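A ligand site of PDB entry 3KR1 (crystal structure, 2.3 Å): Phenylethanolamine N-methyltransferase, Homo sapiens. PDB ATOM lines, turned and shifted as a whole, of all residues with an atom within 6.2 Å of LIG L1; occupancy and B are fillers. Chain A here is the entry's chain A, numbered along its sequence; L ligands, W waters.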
ATOM      1  N   ALA A  24       0.886  -6.318 -17.352  1.00  0.00           N
ATOM      2  CA  ALA A  24      -0.134  -5.670 -16.521  1.00  0.00           C
ATOM      3  C   ALA A  24      -0.225  -6.327 -15.147  1.00  0.00           C
ATOM      4  O   ALA A  24      -0.158  -5.638 -14.131  1.00  0.00           O
ATOM      5  CB  ALA A  24      -1.484  -5.702 -17.221  1.00  0.00           C
ATOM      6  N   TYR A  27       1.701  -5.260 -12.292  1.00  0.00           N
ATOM      7  CA  TYR A  27       1.288  -4.146 -11.438  1.00  0.00           C
ATOM      8  C   TYR A  27       0.634  -4.585 -10.141  1.00  0.00           C
ATOM      9  O   TYR A  27       0.461  -3.786  -9.228  1.00  0.00           O
ATOM     10  CB  TYR A  27       0.390  -3.177 -12.216  1.00  0.00           C
ATOM     11  CG  TYR A  27       1.195  -2.157 -12.963  1.00  0.00           C
ATOM     12  CD1 TYR A  27       1.445  -2.290 -14.317  1.00  0.00           C
ATOM     13  CD2 TYR A  27       1.731  -1.057 -12.304  1.00  0.00           C
ATOM     14  CE1 TYR A  27       2.189  -1.357 -15.007  1.00  0.00           C
ATOM     15  CE2 TYR A  27       2.484  -0.125 -12.967  1.00  0.00           C
ATOM     16  CZ  TYR A  27       2.712  -0.278 -14.322  1.00  0.00           C
ATOM     17  OH  TYR A  27       3.454   0.662 -14.988  1.00  0.00           O
ATOM     18  N   PHE A  30       3.234  -4.080  -7.576  1.00  0.00           N
ATOM     19  CA  PHE A  30       3.652  -2.692  -7.410  1.00  0.00           C
ATOM     20  C   PHE A  30       3.545  -2.213  -5.964  1.00  0.00           C
ATOM     21  O   PHE A  30       2.466  -2.222  -5.372  1.00  0.00           O
ATOM     22  CB  PHE A  30       2.767  -1.824  -8.314  1.00  0.00           C
ATOM     23  CG  PHE A  30       3.184  -0.373  -8.379  1.00  0.00           C
ATOM     24  CD1 PHE A  30       3.876   0.114  -9.486  1.00  0.00           C
ATOM     25  CD2 PHE A  30       2.849   0.502  -7.370  1.00  0.00           C
ATOM     26  CE1 PHE A  30       4.240   1.448  -9.556  1.00  0.00           C
ATOM     27  CE2 PHE A  30       3.212   1.836  -7.441  1.00  0.00           C
ATOM     28  CZ  PHE A  30       3.908   2.309  -8.534  1.00  0.00           C
ATOM     29  N   TYR A  35       8.099   2.768  -4.897  1.00  0.00           N
ATOM     30  CA  TYR A  35       8.038   3.679  -6.034  1.00  0.00           C
ATOM     31  C   TYR A  35       8.380   5.110  -5.609  1.00  0.00           C
ATOM     32  O   TYR A  35       9.191   5.776  -6.260  1.00  0.00           O
ATOM     33  CB  TYR A  35       6.649   3.650  -6.690  1.00  0.00           C
ATOM     34  CG  TYR A  35       6.534   4.594  -7.867  1.00  0.00           C
ATOM     35  CD1 TYR A  35       7.162   4.312  -9.079  1.00  0.00           C
ATOM     36  CD2 TYR A  35       5.786   5.763  -7.773  1.00  0.00           C
ATOM     37  CE1 TYR A  35       7.047   5.165 -10.146  1.00  0.00           C
ATOM     38  CE2 TYR A  35       5.673   6.622  -8.832  1.00  0.00           C
ATOM     39  CZ  TYR A  35       6.307   6.319 -10.024  1.00  0.00           C
ATOM     40  OH  TYR A  35       6.192   7.186 -11.091  1.00  0.00           O
ATOM     41  N   ASN A  39      11.891   7.274  -6.824  1.00  0.00           N
ATOM     42  CA  ASN A  39      11.735   8.357  -7.782  1.00  0.00           C
ATOM     43  C   ASN A  39      11.534   9.745  -7.170  1.00  0.00           C
ATOM     44  O   ASN A  39      11.736  10.760  -7.849  1.00  0.00           O
ATOM     45  CB  ASN A  39      10.577   8.040  -8.719  1.00  0.00           C
ATOM     46  CG  ASN A  39      10.842   6.823  -9.583  1.00  0.00           C
ATOM     47  OD1 ASN A  39      11.768   6.820 -10.398  1.00  0.00           O
ATOM     48  ND2 ASN A  39      10.034   5.785  -9.419  1.00  0.00           N
ATOM     49  N   TYR A  40      11.136   9.790  -5.915  1.00  0.00           N
ATOM     50  CA  TYR A  40      10.783  11.068  -5.289  1.00  0.00           C
ATOM     51  C   TYR A  40      11.486  11.301  -3.964  1.00  0.00           C
ATOM     52  O   TYR A  40      11.114  12.178  -3.182  1.00  0.00           O
ATOM     53  CB  TYR A  40       9.269  11.181  -5.180  1.00  0.00           C
ATOM     54  CG  TYR A  40       8.628  11.106  -6.546  1.00  0.00           C
ATOM     55  CD1 TYR A  40       8.049   9.933  -7.004  1.00  0.00           C
ATOM     56  CD2 TYR A  40       8.668  12.196  -7.400  1.00  0.00           C
ATOM     57  CE1 TYR A  40       7.489   9.867  -8.263  1.00  0.00           C
ATOM     58  CE2 TYR A  40       8.110  12.137  -8.653  1.00  0.00           C
ATOM     59  CZ  TYR A  40       7.520  10.972  -9.084  1.00  0.00           C
ATOM     60  OH  TYR A  40       6.962  10.934 -10.343  1.00  0.00           O
ATOM     61  N   LYS A  57      10.660  19.351 -13.975  1.00  0.00           N
ATOM     62  CA  LYS A  57       9.259  18.964 -14.102  1.00  0.00           C
ATOM     63  C   LYS A  57       8.312  20.038 -13.551  1.00  0.00           C
ATOM     64  O   LYS A  57       7.325  20.390 -14.204  1.00  0.00           O
ATOM     65  CB  LYS A  57       8.986  17.628 -13.404  1.00  0.00           C
ATOM     66  CG  LYS A  57       9.383  16.416 -14.223  1.00  0.00           C
ATOM     67  CD  LYS A  57       8.838  15.134 -13.617  1.00  0.00           C
ATOM     68  CE  LYS A  57       9.503  14.825 -12.282  1.00  0.00           C
ATOM     69  NZ  LYS A  57       9.015  13.538 -11.725  1.00  0.00           N
ATOM     70  N   ASP A  77      -6.576  13.916 -13.402  1.00  0.00           N
ATOM     71  CA  ASP A  77      -5.212  13.411 -13.399  1.00  0.00           C
ATOM     72  C   ASP A  77      -5.219  11.913 -13.702  1.00  0.00           C
ATOM     73  O   ASP A  77      -5.792  11.124 -12.949  1.00  0.00           O
ATOM     74  CB  ASP A  77      -4.550  13.697 -12.051  1.00  0.00           C
ATOM     75  CG  ASP A  77      -3.104  13.285 -12.014  1.00  0.00           C
ATOM     76  OD1 ASP A  77      -2.416  13.405 -13.052  1.00  0.00           O
ATOM     77  OD2 ASP A  77      -2.637  12.832 -10.942  1.00  0.00           O
ATOM     78  N   ILE A  78      -4.594  11.533 -14.809  1.00  0.00           N
ATOM     79  CA  ILE A  78      -4.632  10.157 -15.287  1.00  0.00           C
ATOM     80  C   ILE A  78      -3.458   9.322 -14.782  1.00  0.00           C
ATOM     81  O   ILE A  78      -2.307   9.575 -15.131  1.00  0.00           O
ATOM     82  CB  ILE A  78      -4.588  10.094 -16.823  1.00  0.00           C
ATOM     83  CG1 ILE A  78      -5.708  10.953 -17.421  1.00  0.00           C
ATOM     84  CG2 ILE A  78      -4.675   8.658 -17.306  1.00  0.00           C
ATOM     85  CD1 ILE A  78      -7.088  10.405 -17.177  1.00  0.00           C
ATOM     86  N   GLY A  79      -3.762   8.308 -13.969  1.00  0.00           N
ATOM     87  CA  GLY A  79      -2.724   7.426 -13.448  1.00  0.00           C
ATOM     88  C   GLY A  79      -1.852   8.162 -12.449  1.00  0.00           C
ATOM     89  O   GLY A  79      -0.627   8.191 -12.567  1.00  0.00           O
ATOM     90  N   SER A  80      -2.515   8.764 -11.467  1.00  0.00           N
ATOM     91  CA  SER A  80      -1.842   9.558 -10.442  1.00  0.00           C
ATOM     92  C   SER A  80      -0.792   8.755  -9.692  1.00  0.00           C
ATOM     93  O   SER A  80       0.214   9.293  -9.237  1.00  0.00           O
ATOM     94  CB  SER A  80      -2.867  10.115  -9.454  1.00  0.00           C
ATOM     95  OG  SER A  80      -3.945  10.736 -10.124  1.00  0.00           O
ATOM     96  N   GLY A  81      -1.038   7.448  -9.564  1.00  0.00           N
ATOM     97  CA  GLY A  81      -0.244   6.615  -8.687  1.00  0.00           C
ATOM     98  C   GLY A  81      -0.350   7.199  -7.292  1.00  0.00           C
ATOM     99  O   GLY A  81      -1.413   7.692  -6.914  1.00  0.00           O
ATOM    100  N   PRO A  82       0.733   7.138  -6.516  1.00  0.00           N
ATOM    101  CA  PRO A  82       0.725   7.736  -5.177  1.00  0.00           C
ATOM    102  C   PRO A  82       1.354   9.115  -5.137  1.00  0.00           C
ATOM    103  O   PRO A  82       1.820   9.520  -4.071  1.00  0.00           O
ATOM    104  CB  PRO A  82       1.580   6.756  -4.399  1.00  0.00           C
ATOM    105  CG  PRO A  82       2.659   6.422  -5.372  1.00  0.00           C
ATOM    106  CD  PRO A  82       2.007   6.425  -6.755  1.00  0.00           C
ATOM    107  N   THR A  83       1.401   9.835  -6.255  1.00  0.00           N
ATOM    108  CA  THR A  83       2.028  11.149  -6.268  1.00  0.00           C
ATOM    109  C   THR A  83       1.053  12.291  -6.484  1.00  0.00           C
ATOM    110  O   THR A  83      -0.011  12.125  -7.091  1.00  0.00           O
ATOM    111  CB  THR A  83       3.173  11.249  -7.300  1.00  0.00           C
ATOM    112  OG1 THR A  83       2.630  11.281  -8.623  1.00  0.00           O
ATOM    113  CG2 THR A  83       4.115  10.060  -7.171  1.00  0.00           C
ATOM    114  N   TYR A  85       2.591  15.770  -6.824  1.00  0.00           N
ATOM    115  CA  TYR A  85       3.385  16.885  -7.318  1.00  0.00           C
ATOM    116  C   TYR A  85       2.857  17.418  -8.645  1.00  0.00           C
ATOM    117  O   TYR A  85       2.931  18.624  -8.910  1.00  0.00           O
ATOM    118  CB  TYR A  85       4.840  16.478  -7.502  1.00  0.00           C
ATOM    119  CG  TYR A  85       5.064  15.588  -8.705  1.00  0.00           C
ATOM    120  CD1 TYR A  85       5.408  16.122  -9.937  1.00  0.00           C
ATOM    121  CD2 TYR A  85       4.908  14.218  -8.609  1.00  0.00           C
ATOM    122  CE1 TYR A  85       5.600  15.320 -11.037  1.00  0.00           C
ATOM    123  CE2 TYR A  85       5.104  13.402  -9.696  1.00  0.00           C
ATOM    124  CZ  TYR A  85       5.447  13.957 -10.905  1.00  0.00           C
ATOM    125  OH  TYR A  85       5.640  13.134 -11.998  1.00  0.00           O
ATOM    126  N   GLN A  86       2.350  16.514  -9.474  1.00  0.00           N
ATOM    127  CA  GLN A  86       1.918  16.871 -10.822  1.00  0.00           C
ATOM    128  C   GLN A  86       0.720  17.832 -10.815  1.00  0.00           C
ATOM    129  O   GLN A  86       0.344  18.363 -11.857  1.00  0.00           O
ATOM    130  CB  GLN A  86       1.610  15.619 -11.645  1.00  0.00           C
ATOM    131  CG  GLN A  86       0.438  14.794 -11.141  1.00  0.00           C
ATOM    132  CD  GLN A  86       0.865  13.713 -10.165  1.00  0.00           C
ATOM    133  OE1 GLN A  86       1.862  13.849  -9.468  1.00  0.00           O
ATOM    134  NE2 GLN A  86       0.081  12.637 -10.108  1.00  0.00           N
ATOM    135  N   ASP A 101      -6.209   6.139 -10.189  1.00  0.00           N
ATOM    136  CA  ASP A 101      -5.225   5.100 -10.461  1.00  0.00           C
ATOM    137  C   ASP A 101      -5.876   3.736 -10.627  1.00  0.00           C
ATOM    138  O   ASP A 101      -7.004   3.503 -10.188  1.00  0.00           O
ATOM    139  CB  ASP A 101      -4.118   5.032  -9.401  1.00  0.00           C
ATOM    140  CG  ASP A 101      -2.874   4.334  -9.914  1.00  0.00           C
ATOM    141  OD1 ASP A 101      -2.277   4.829 -10.898  1.00  0.00           O
ATOM    142  OD2 ASP A 101      -2.494   3.281  -9.355  1.00  0.00           O
ATOM    143  N   PHE A 102      -5.156   2.849 -11.291  1.00  0.00           N
ATOM    144  CA  PHE A 102      -5.598   1.483 -11.560  1.00  0.00           C
ATOM    145  C   PHE A 102      -5.544   0.651 -10.278  1.00  0.00           C
ATOM    146  O   PHE A 102      -6.389  -0.207 -10.046  1.00  0.00           O
ATOM    147  CB  PHE A 102      -4.706   0.885 -12.645  1.00  0.00           C
ATOM    148  CG  PHE A 102      -5.004  -0.556 -12.973  1.00  0.00           C
ATOM    149  CD1 PHE A 102      -6.092  -0.899 -13.763  1.00  0.00           C
ATOM    150  CD2 PHE A 102      -4.168  -1.551 -12.519  1.00  0.00           C
ATOM    151  CE1 PHE A 102      -6.343  -2.216 -14.075  1.00  0.00           C
ATOM    152  CE2 PHE A 102      -4.418  -2.875 -12.824  1.00  0.00           C
ATOM    153  CZ  PHE A 102      -5.502  -3.211 -13.607  1.00  0.00           C
ATOM    154  N   LEU A 103      -4.549   0.937  -9.435  1.00  0.00           N
ATOM    155  CA  LEU A 103      -4.321   0.169  -8.218  1.00  0.00           C
ATOM    156  C   LEU A 103      -5.002   0.767  -6.982  1.00  0.00           C
ATOM    157  O   LEU A 103      -4.984   1.987  -6.771  1.00  0.00           O
ATOM    158  CB  LEU A 103      -2.826   0.018  -7.947  1.00  0.00           C
ATOM    159  CG  LEU A 103      -2.042  -0.770  -8.998  1.00  0.00           C
ATOM    160  CD1 LEU A 103      -0.597  -0.945  -8.559  1.00  0.00           C
ATOM    161  CD2 LEU A 103      -2.696  -2.120  -9.238  1.00  0.00           C
ATOM    162  N   ASN A 106      -2.438   2.381  -4.458  1.00  0.00           N
ATOM    163  CA  ASN A 106      -2.088   3.757  -4.793  1.00  0.00           C
ATOM    164  C   ASN A 106      -3.168   4.754  -4.361  1.00  0.00           C
ATOM    165  O   ASN A 106      -2.862   5.834  -3.841  1.00  0.00           O
ATOM    166  CB  ASN A 106      -1.801   3.896  -6.282  1.00  0.00           C
ATOM    167  CG  ASN A 106      -0.387   3.491  -6.646  1.00  0.00           C
ATOM    168  OD1 ASN A 106      -0.104   3.115  -7.792  1.00  0.00           O
ATOM    169  ND2 ASN A 106       0.517   3.551  -5.679  1.00  0.00           N
ATOM    170  N   ILE A 157      -9.241   3.547 -12.562  1.00  0.00           N
ATOM    171  CA  ILE A 157      -9.182   3.859 -13.984  1.00  0.00           C
ATOM    172  C   ILE A 157      -8.350   2.821 -14.720  1.00  0.00           C
ATOM    173  O   ILE A 157      -7.420   2.239 -14.148  1.00  0.00           O
ATOM    174  CB  ILE A 157      -8.596   5.268 -14.228  1.00  0.00           C
ATOM    175  CG1 ILE A 157      -8.669   5.646 -15.708  1.00  0.00           C
ATOM    176  CG2 ILE A 157      -7.176   5.336 -13.732  1.00  0.00           C
ATOM    177  CD1 ILE A 157      -8.241   7.073 -16.009  1.00  0.00           C
ATOM    178  N   ASP A 158      -8.700   2.562 -15.973  1.00  0.00           N
ATOM    179  CA  ASP A 158      -7.919   1.690 -16.830  1.00  0.00           C
ATOM    180  C   ASP A 158      -7.880   2.302 -18.224  1.00  0.00           C
ATOM    181  O   ASP A 158      -8.881   2.272 -18.955  1.00  0.00           O
ATOM    182  CB  ASP A 158      -8.533   0.289 -16.883  1.00  0.00           C
ATOM    183  CG  ASP A 158      -7.745  -0.661 -17.766  1.00  0.00           C
ATOM    184  OD1 ASP A 158      -6.807  -0.204 -18.465  1.00  0.00           O
ATOM    185  OD2 ASP A 158      -8.054  -1.865 -17.779  1.00  0.00           O
ATOM    186  N   VAL A 159      -6.735   2.867 -18.596  1.00  0.00           N
ATOM    187  CA  VAL A 159      -6.606   3.558 -19.870  1.00  0.00           C
ATOM    188  C   VAL A 159      -6.700   2.593 -21.054  1.00  0.00           C
ATOM    189  O   VAL A 159      -6.761   3.030 -22.207  1.00  0.00           O
ATOM    190  CB  VAL A 159      -5.301   4.362 -19.956  1.00  0.00           C
ATOM    191  CG1 VAL A 159      -5.265   5.430 -18.870  1.00  0.00           C
ATOM    192  CG2 VAL A 159      -4.094   3.436 -19.824  1.00  0.00           C
ATOM    193  N   HIS A 160      -6.714   1.298 -20.781  1.00  0.00           N
ATOM    194  CA  HIS A 160      -6.839   0.308 -21.835  1.00  0.00           C
ATOM    195  C   HIS A 160      -8.283   0.150 -22.288  1.00  0.00           C
ATOM    196  O   HIS A 160      -8.563  -0.390 -23.369  1.00  0.00           O
ATOM    197  CB  HIS A 160      -6.277  -1.042 -21.390  1.00  0.00           C
ATOM    198  CG  HIS A 160      -4.789  -1.038 -21.203  1.00  0.00           C
ATOM    199  ND1 HIS A 160      -3.927  -0.512 -22.135  1.00  0.00           N
ATOM    200  CD2 HIS A 160      -4.015  -1.500 -20.192  1.00  0.00           C
ATOM    201  CE1 HIS A 160      -2.686  -0.644 -21.715  1.00  0.00           C
ATOM    202  NE2 HIS A 160      -2.704  -1.245 -20.538  1.00  0.00           N
ATOM    203  N   SER A 180      -1.322  13.943 -17.007  1.00  0.00           N
ATOM    204  CA  SER A 180      -0.889  12.557 -16.832  1.00  0.00           C
ATOM    205  C   SER A 180       0.625  12.445 -16.881  1.00  0.00           C
ATOM    206  O   SER A 180       1.268  12.958 -17.798  1.00  0.00           O
ATOM    207  CB  SER A 180      -1.526  11.640 -17.879  1.00  0.00           C
ATOM    208  OG  SER A 180      -1.093  10.312 -17.688  1.00  0.00           O
ATOM    209  N   ALA A 181       1.194  11.771 -15.893  1.00  0.00           N
ATOM    210  CA  ALA A 181       2.647  11.679 -15.786  1.00  0.00           C
ATOM    211  C   ALA A 181       3.136  10.254 -15.564  1.00  0.00           C
ATOM    212  O   ALA A 181       2.765   9.593 -14.594  1.00  0.00           O
ATOM    213  CB  ALA A 181       3.143  12.585 -14.683  1.00  0.00           C
ATOM    214  N   PHE A 182       3.993   9.795 -16.476  1.00  0.00           N
ATOM    215  CA  PHE A 182       4.616   8.480 -16.381  1.00  0.00           C
ATOM    216  C   PHE A 182       3.614   7.335 -16.324  1.00  0.00           C
ATOM    217  O   PHE A 182       3.880   6.312 -15.702  1.00  0.00           O
ATOM    218  CB  PHE A 182       5.537   8.399 -15.152  1.00  0.00           C
ATOM    219  CG  PHE A 182       6.617   9.439 -15.148  1.00  0.00           C
ATOM    220  CD1 PHE A 182       6.517  10.551 -14.336  1.00  0.00           C
ATOM    221  CD2 PHE A 182       7.735   9.294 -15.958  1.00  0.00           C
ATOM    222  CE1 PHE A 182       7.520  11.512 -14.321  1.00  0.00           C
ATOM    223  CE2 PHE A 182       8.736  10.241 -15.943  1.00  0.00           C
ATOM    224  CZ  PHE A 182       8.628  11.354 -15.128  1.00  0.00           C
ATOM    225  N   CYS A 183       2.472   7.500 -16.987  1.00  0.00           N
ATOM    226  CA  CYS A 183       1.476   6.439 -16.991  1.00  0.00           C
ATOM    227  C   CYS A 183       1.469   5.644 -18.299  1.00  0.00           C
ATOM    228  O   CYS A 183       1.851   4.481 -18.319  1.00  0.00           O
ATOM    229  CB  CYS A 183       0.074   6.985 -16.719  1.00  0.00           C
ATOM    230  SG  CYS A 183      -1.192   5.696 -16.626  1.00  0.00           S
ATOM    231  N   ALA A 186       4.258   3.608 -19.388  1.00  0.00           N
ATOM    232  CA  ALA A 186       4.536   2.659 -18.320  1.00  0.00           C
ATOM    233  C   ALA A 186       3.515   1.515 -18.227  1.00  0.00           C
ATOM    234  O   ALA A 186       3.714   0.555 -17.476  1.00  0.00           O
ATOM    235  CB  ALA A 186       4.666   3.388 -16.982  1.00  0.00           C
ATOM    236  N   VAL A 187       2.430   1.619 -18.987  1.00  0.00           N
ATOM    237  CA  VAL A 187       1.399   0.589 -18.978  1.00  0.00           C
ATOM    238  C   VAL A 187       1.126   0.026 -20.368  1.00  0.00           C
ATOM    239  O   VAL A 187       0.173  -0.727 -20.561  1.00  0.00           O
ATOM    240  CB  VAL A 187       0.069   1.117 -18.401  1.00  0.00           C
ATOM    241  CG1 VAL A 187       0.291   1.790 -17.058  1.00  0.00           C
ATOM    242  CG2 VAL A 187      -0.616   2.069 -19.388  1.00  0.00           C
ATOM    243  N   TYR A 222      11.239  -0.405 -15.144  1.00  0.00           N
ATOM    244  CA  TYR A 222      11.489   0.252 -13.870  1.00  0.00           C
ATOM    245  C   TYR A 222      10.999  -0.633 -12.736  1.00  0.00           C
ATOM    246  O   TYR A 222      10.142  -1.493 -12.934  1.00  0.00           O
ATOM    247  CB  TYR A 222      10.862   1.653 -13.813  1.00  0.00           C
ATOM    248  CG  TYR A 222       9.360   1.680 -13.680  1.00  0.00           C
ATOM    249  CD1 TYR A 222       8.755   1.995 -12.469  1.00  0.00           C
ATOM    250  CD2 TYR A 222       8.545   1.414 -14.773  1.00  0.00           C
ATOM    251  CE1 TYR A 222       7.378   2.041 -12.349  1.00  0.00           C
ATOM    252  CE2 TYR A 222       7.174   1.452 -14.663  1.00  0.00           C
ATOM    253  CZ  TYR A 222       6.593   1.766 -13.444  1.00  0.00           C
ATOM    254  OH  TYR A 222       5.222   1.804 -13.334  1.00  0.00           O
HETATM  255  N1  LIG L   1       1.706   9.738 -12.060  1.00  0.00           N
HETATM  256  C1  LIG L   1       2.670   9.255 -11.079  1.00  0.00           C
HETATM  257  C2  LIG L   1       2.720   7.727 -11.028  1.00  0.00           C
HETATM  258  C3  LIG L   1       3.206   7.058 -12.317  1.00  0.00           C
HETATM  259  S1  LIG L   1       3.518   5.279 -12.070  1.00  0.00           S
HETATM  260  C4  LIG L   1       4.042   9.889 -11.333  1.00  0.00           C
HETATM  261  O1  LIG L   1       4.925   9.488 -10.659  1.00  0.00           O
HETATM  262  O2  LIG L   1       4.028  11.134 -11.979  1.00  0.00           O
HETATM  263  C5  LIG L   1       2.378   4.546 -13.290  1.00  0.00           C
HETATM  264  C6  LIG L   1       0.953   4.301 -12.786  1.00  0.00           C
HETATM  265  O3  LIG L   1       0.244   3.617 -13.758  1.00  0.00           O
HETATM  266  C7  LIG L   1       0.905   3.348 -11.589  1.00  0.00           C
HETATM  267  O4  LIG L   1       0.386   4.053 -10.490  1.00  0.00           O
HETATM  268  C8  LIG L   1       0.043   2.346 -11.983  1.00  0.00           C
HETATM  269  O5  LIG L   1      -0.798   1.904 -10.950  1.00  0.00           O
HETATM  270  C9  LIG L   1      -0.716   2.934 -13.041  1.00  0.00           C
HETATM  271  N2  LIG L   1      -1.377   1.963 -13.900  1.00  0.00           N
HETATM  272  C10 LIG L   1      -1.049   0.689 -14.083  1.00  0.00           C
HETATM  273  N3  LIG L   1      -1.905   0.144 -15.017  1.00  0.00           N
HETATM  274  C11 LIG L   1      -2.780   1.128 -15.398  1.00  0.00           C
HETATM  275  C12 LIG L   1      -3.822   1.135 -16.286  1.00  0.00           C
HETATM  276  N4  LIG L   1      -4.167  -0.063 -17.013  1.00  0.00           N
HETATM  277  N5  LIG L   1      -4.526   2.243 -16.477  1.00  0.00           N
HETATM  278  C13 LIG L   1      -4.205   3.372 -15.804  1.00  0.00           C
HETATM  279  N6  LIG L   1      -3.168   3.365 -14.929  1.00  0.00           N
HETATM  280  C14 LIG L   1      -2.465   2.244 -14.738  1.00  0.00           C
HETATM  281 CL1  LG2 L   2      14.336  10.799 -13.677  1.00  0.00          CL
HETATM  282  C1  LG2 L   2      12.719  10.277 -13.178  1.00  0.00           C
HETATM  283  C2  LG2 L   2      12.027  10.994 -12.213  1.00  0.00           C
HETATM  284  C3  LG2 L   2      10.760  10.601 -11.803  1.00  0.00           C
HETATM  285  C4  LG2 L   2      10.187   9.462 -12.374  1.00  0.00           C
HETATM  286  C5  LG2 L   2      10.877   8.731 -13.339  1.00  0.00           C
HETATM  287  C6  LG2 L   2      12.161   9.151 -13.739  1.00  0.00           C
HETATM  288  N1  LG2 L   2       8.962   8.831 -12.186  1.00  0.00           N
HETATM  289  C7  LG2 L   2       8.890   7.739 -13.005  1.00  0.00           C
HETATM  290  N2  LG2 L   2      10.059   7.669 -13.719  1.00  0.00           N
HETATM  291  N3  LG2 L   2       7.786   6.835 -13.081  1.00  0.00           N
HETATM  292  O   HOH W   1      -0.569  11.472 -13.393  1.00  0.00           O
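The side-chain hydroxyl (OH) of Tyr 85 lies within hydrogen-bond range of the side-chain hydroxyl (OH) of Tyr 40, at 3.1 Å. OD1 of Asp 101 lies within hydrogen-bond range of N of Gly 81, 3.2 Å away. OD2 of Asp 101 lies within hydrogen-bond range of N of Leu 103 (3.1 Å). The backbone carbonyl oxygen of Asp 101 sits at hydrogen-bond distance from the backbone NH of Ile 157. The side-chain carboxylate (OD1) of Asp 158 lies within hydrogen-bond range of the backbone NH (N) of His 160 (2.8 Å). The side-chain hydroxyl (OG) of Ser 80 lies within hydrogen-bond range of the side-chain carboxylate (OD2) of Asp 77 (2.6 Å). OE1 of Gln 86 is in hydrogen-bond range of OG1 of Thr 83 (2.8 Å). The side-chain hydroxyl of Tyr 222 sits at hydrogen-bond distance from the side-chain hydroxyl of Tyr 27 (2.7 Å).
An oxygen (O1) of LIG L1 lies within hydrogen-bond range of the side-chain hydroxyl (OH) of Tyr 40, 2.5 Å away. The side-chain hydroxyl (OH) of Tyr 85 is in hydrogen-bond range of an oxygen (O2) of LIG L1. OH of Tyr 35 lies within hydrogen-bond range of O1 of LIG L1 (2.7 Å). The side-chain carboxylate of Asp 101 lies within hydrogen-bond range of an oxygen (O5) of LIG L1, at 2.7 Å. The backbone carbonyl oxygen of Ala 181 sits at hydrogen-bond distance from a nitrogen (N1) of LIG L1, 2.8 Å away. The backbone carbonyl oxygen (O) of Gly 79 lies within hydrogen-bond range of a nitrogen (N1) of LIG L1 (2.8 Å). The side-chain amide oxygen (OD1) of Asn 106 sits at hydrogen-bond distance from an oxygen (O4) of LIG L1 (2.9 Å). The side-chain carboxylate (OD1) of Asp 158 is in hydrogen-bond range of a nitrogen (N4) of LIG L1 (3.0 Å). O of Ser 80 lies close to N1 of LIG L1, 3.2 Å away. A nitrogen (N5) of LIG L1 sits at hydrogen-bond distance from the backbone NH of Val 159 (3.1 Å). A nitrogen (N6) of LIG L1 lies within hydrogen-bond range of the side-chain sulfur (SG) of Cys 183. The side-chain hydroxyl of Tyr 40 lies within hydrogen-bond range of a nitrogen (N1) of LG2 L2, at 3.4 Å. The side-chain hydroxyl of Tyr 35 sits at hydrogen-bond distance from a nitrogen (N3) of LG2 L2 (2.6 Å).
A sulfur (S1) of LIG L1 sits close to the backbone carbonyl oxygen (O) of Phe 182. CE2 of Tyr 27 touches C8 of LIG L1, at 3.6 Å. CA of Gly 81 touches O4 of LIG L1, at 3.2 Å. Thr 83 touches LIG L1. NE2 of Gln 86 touches N1 of LIG L1, 3.9 Å away. Phe 102 touches LIG L1 (CB to C14, 3.4 Å). CG of Leu 103 touches O5 of LIG L1 (3.5 Å). Ile 157 touches LIG L1. His 160 touches LIG L1 (CD2 to N4, 3.5 Å). CG1 of Val 187 touches N3 of LIG L1 (3.4 Å). Tyr 222 touches LIG L1. Hydrophobic or aromatic side chains within 4 Å of LIG L1: Tyr 27, Tyr 35, Tyr 40, Tyr 85, Phe 102, Leu 103, Val 159, His 160, Ala 181, Phe 182 and Val 187. 22 residues have an atom within 4 Å of LIG L1: Tyr 27, Tyr 35, Tyr 40, Gly 79, Ser 80, Gly 81, Thr 83, Tyr 85, Gln 86, Asp 101, Phe 102, Leu 103, Asn 106, Ile 157, Asp 158, Val 159, His 160, Ala 181, Phe 182, Cys 183, Val 187 and Tyr 222.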
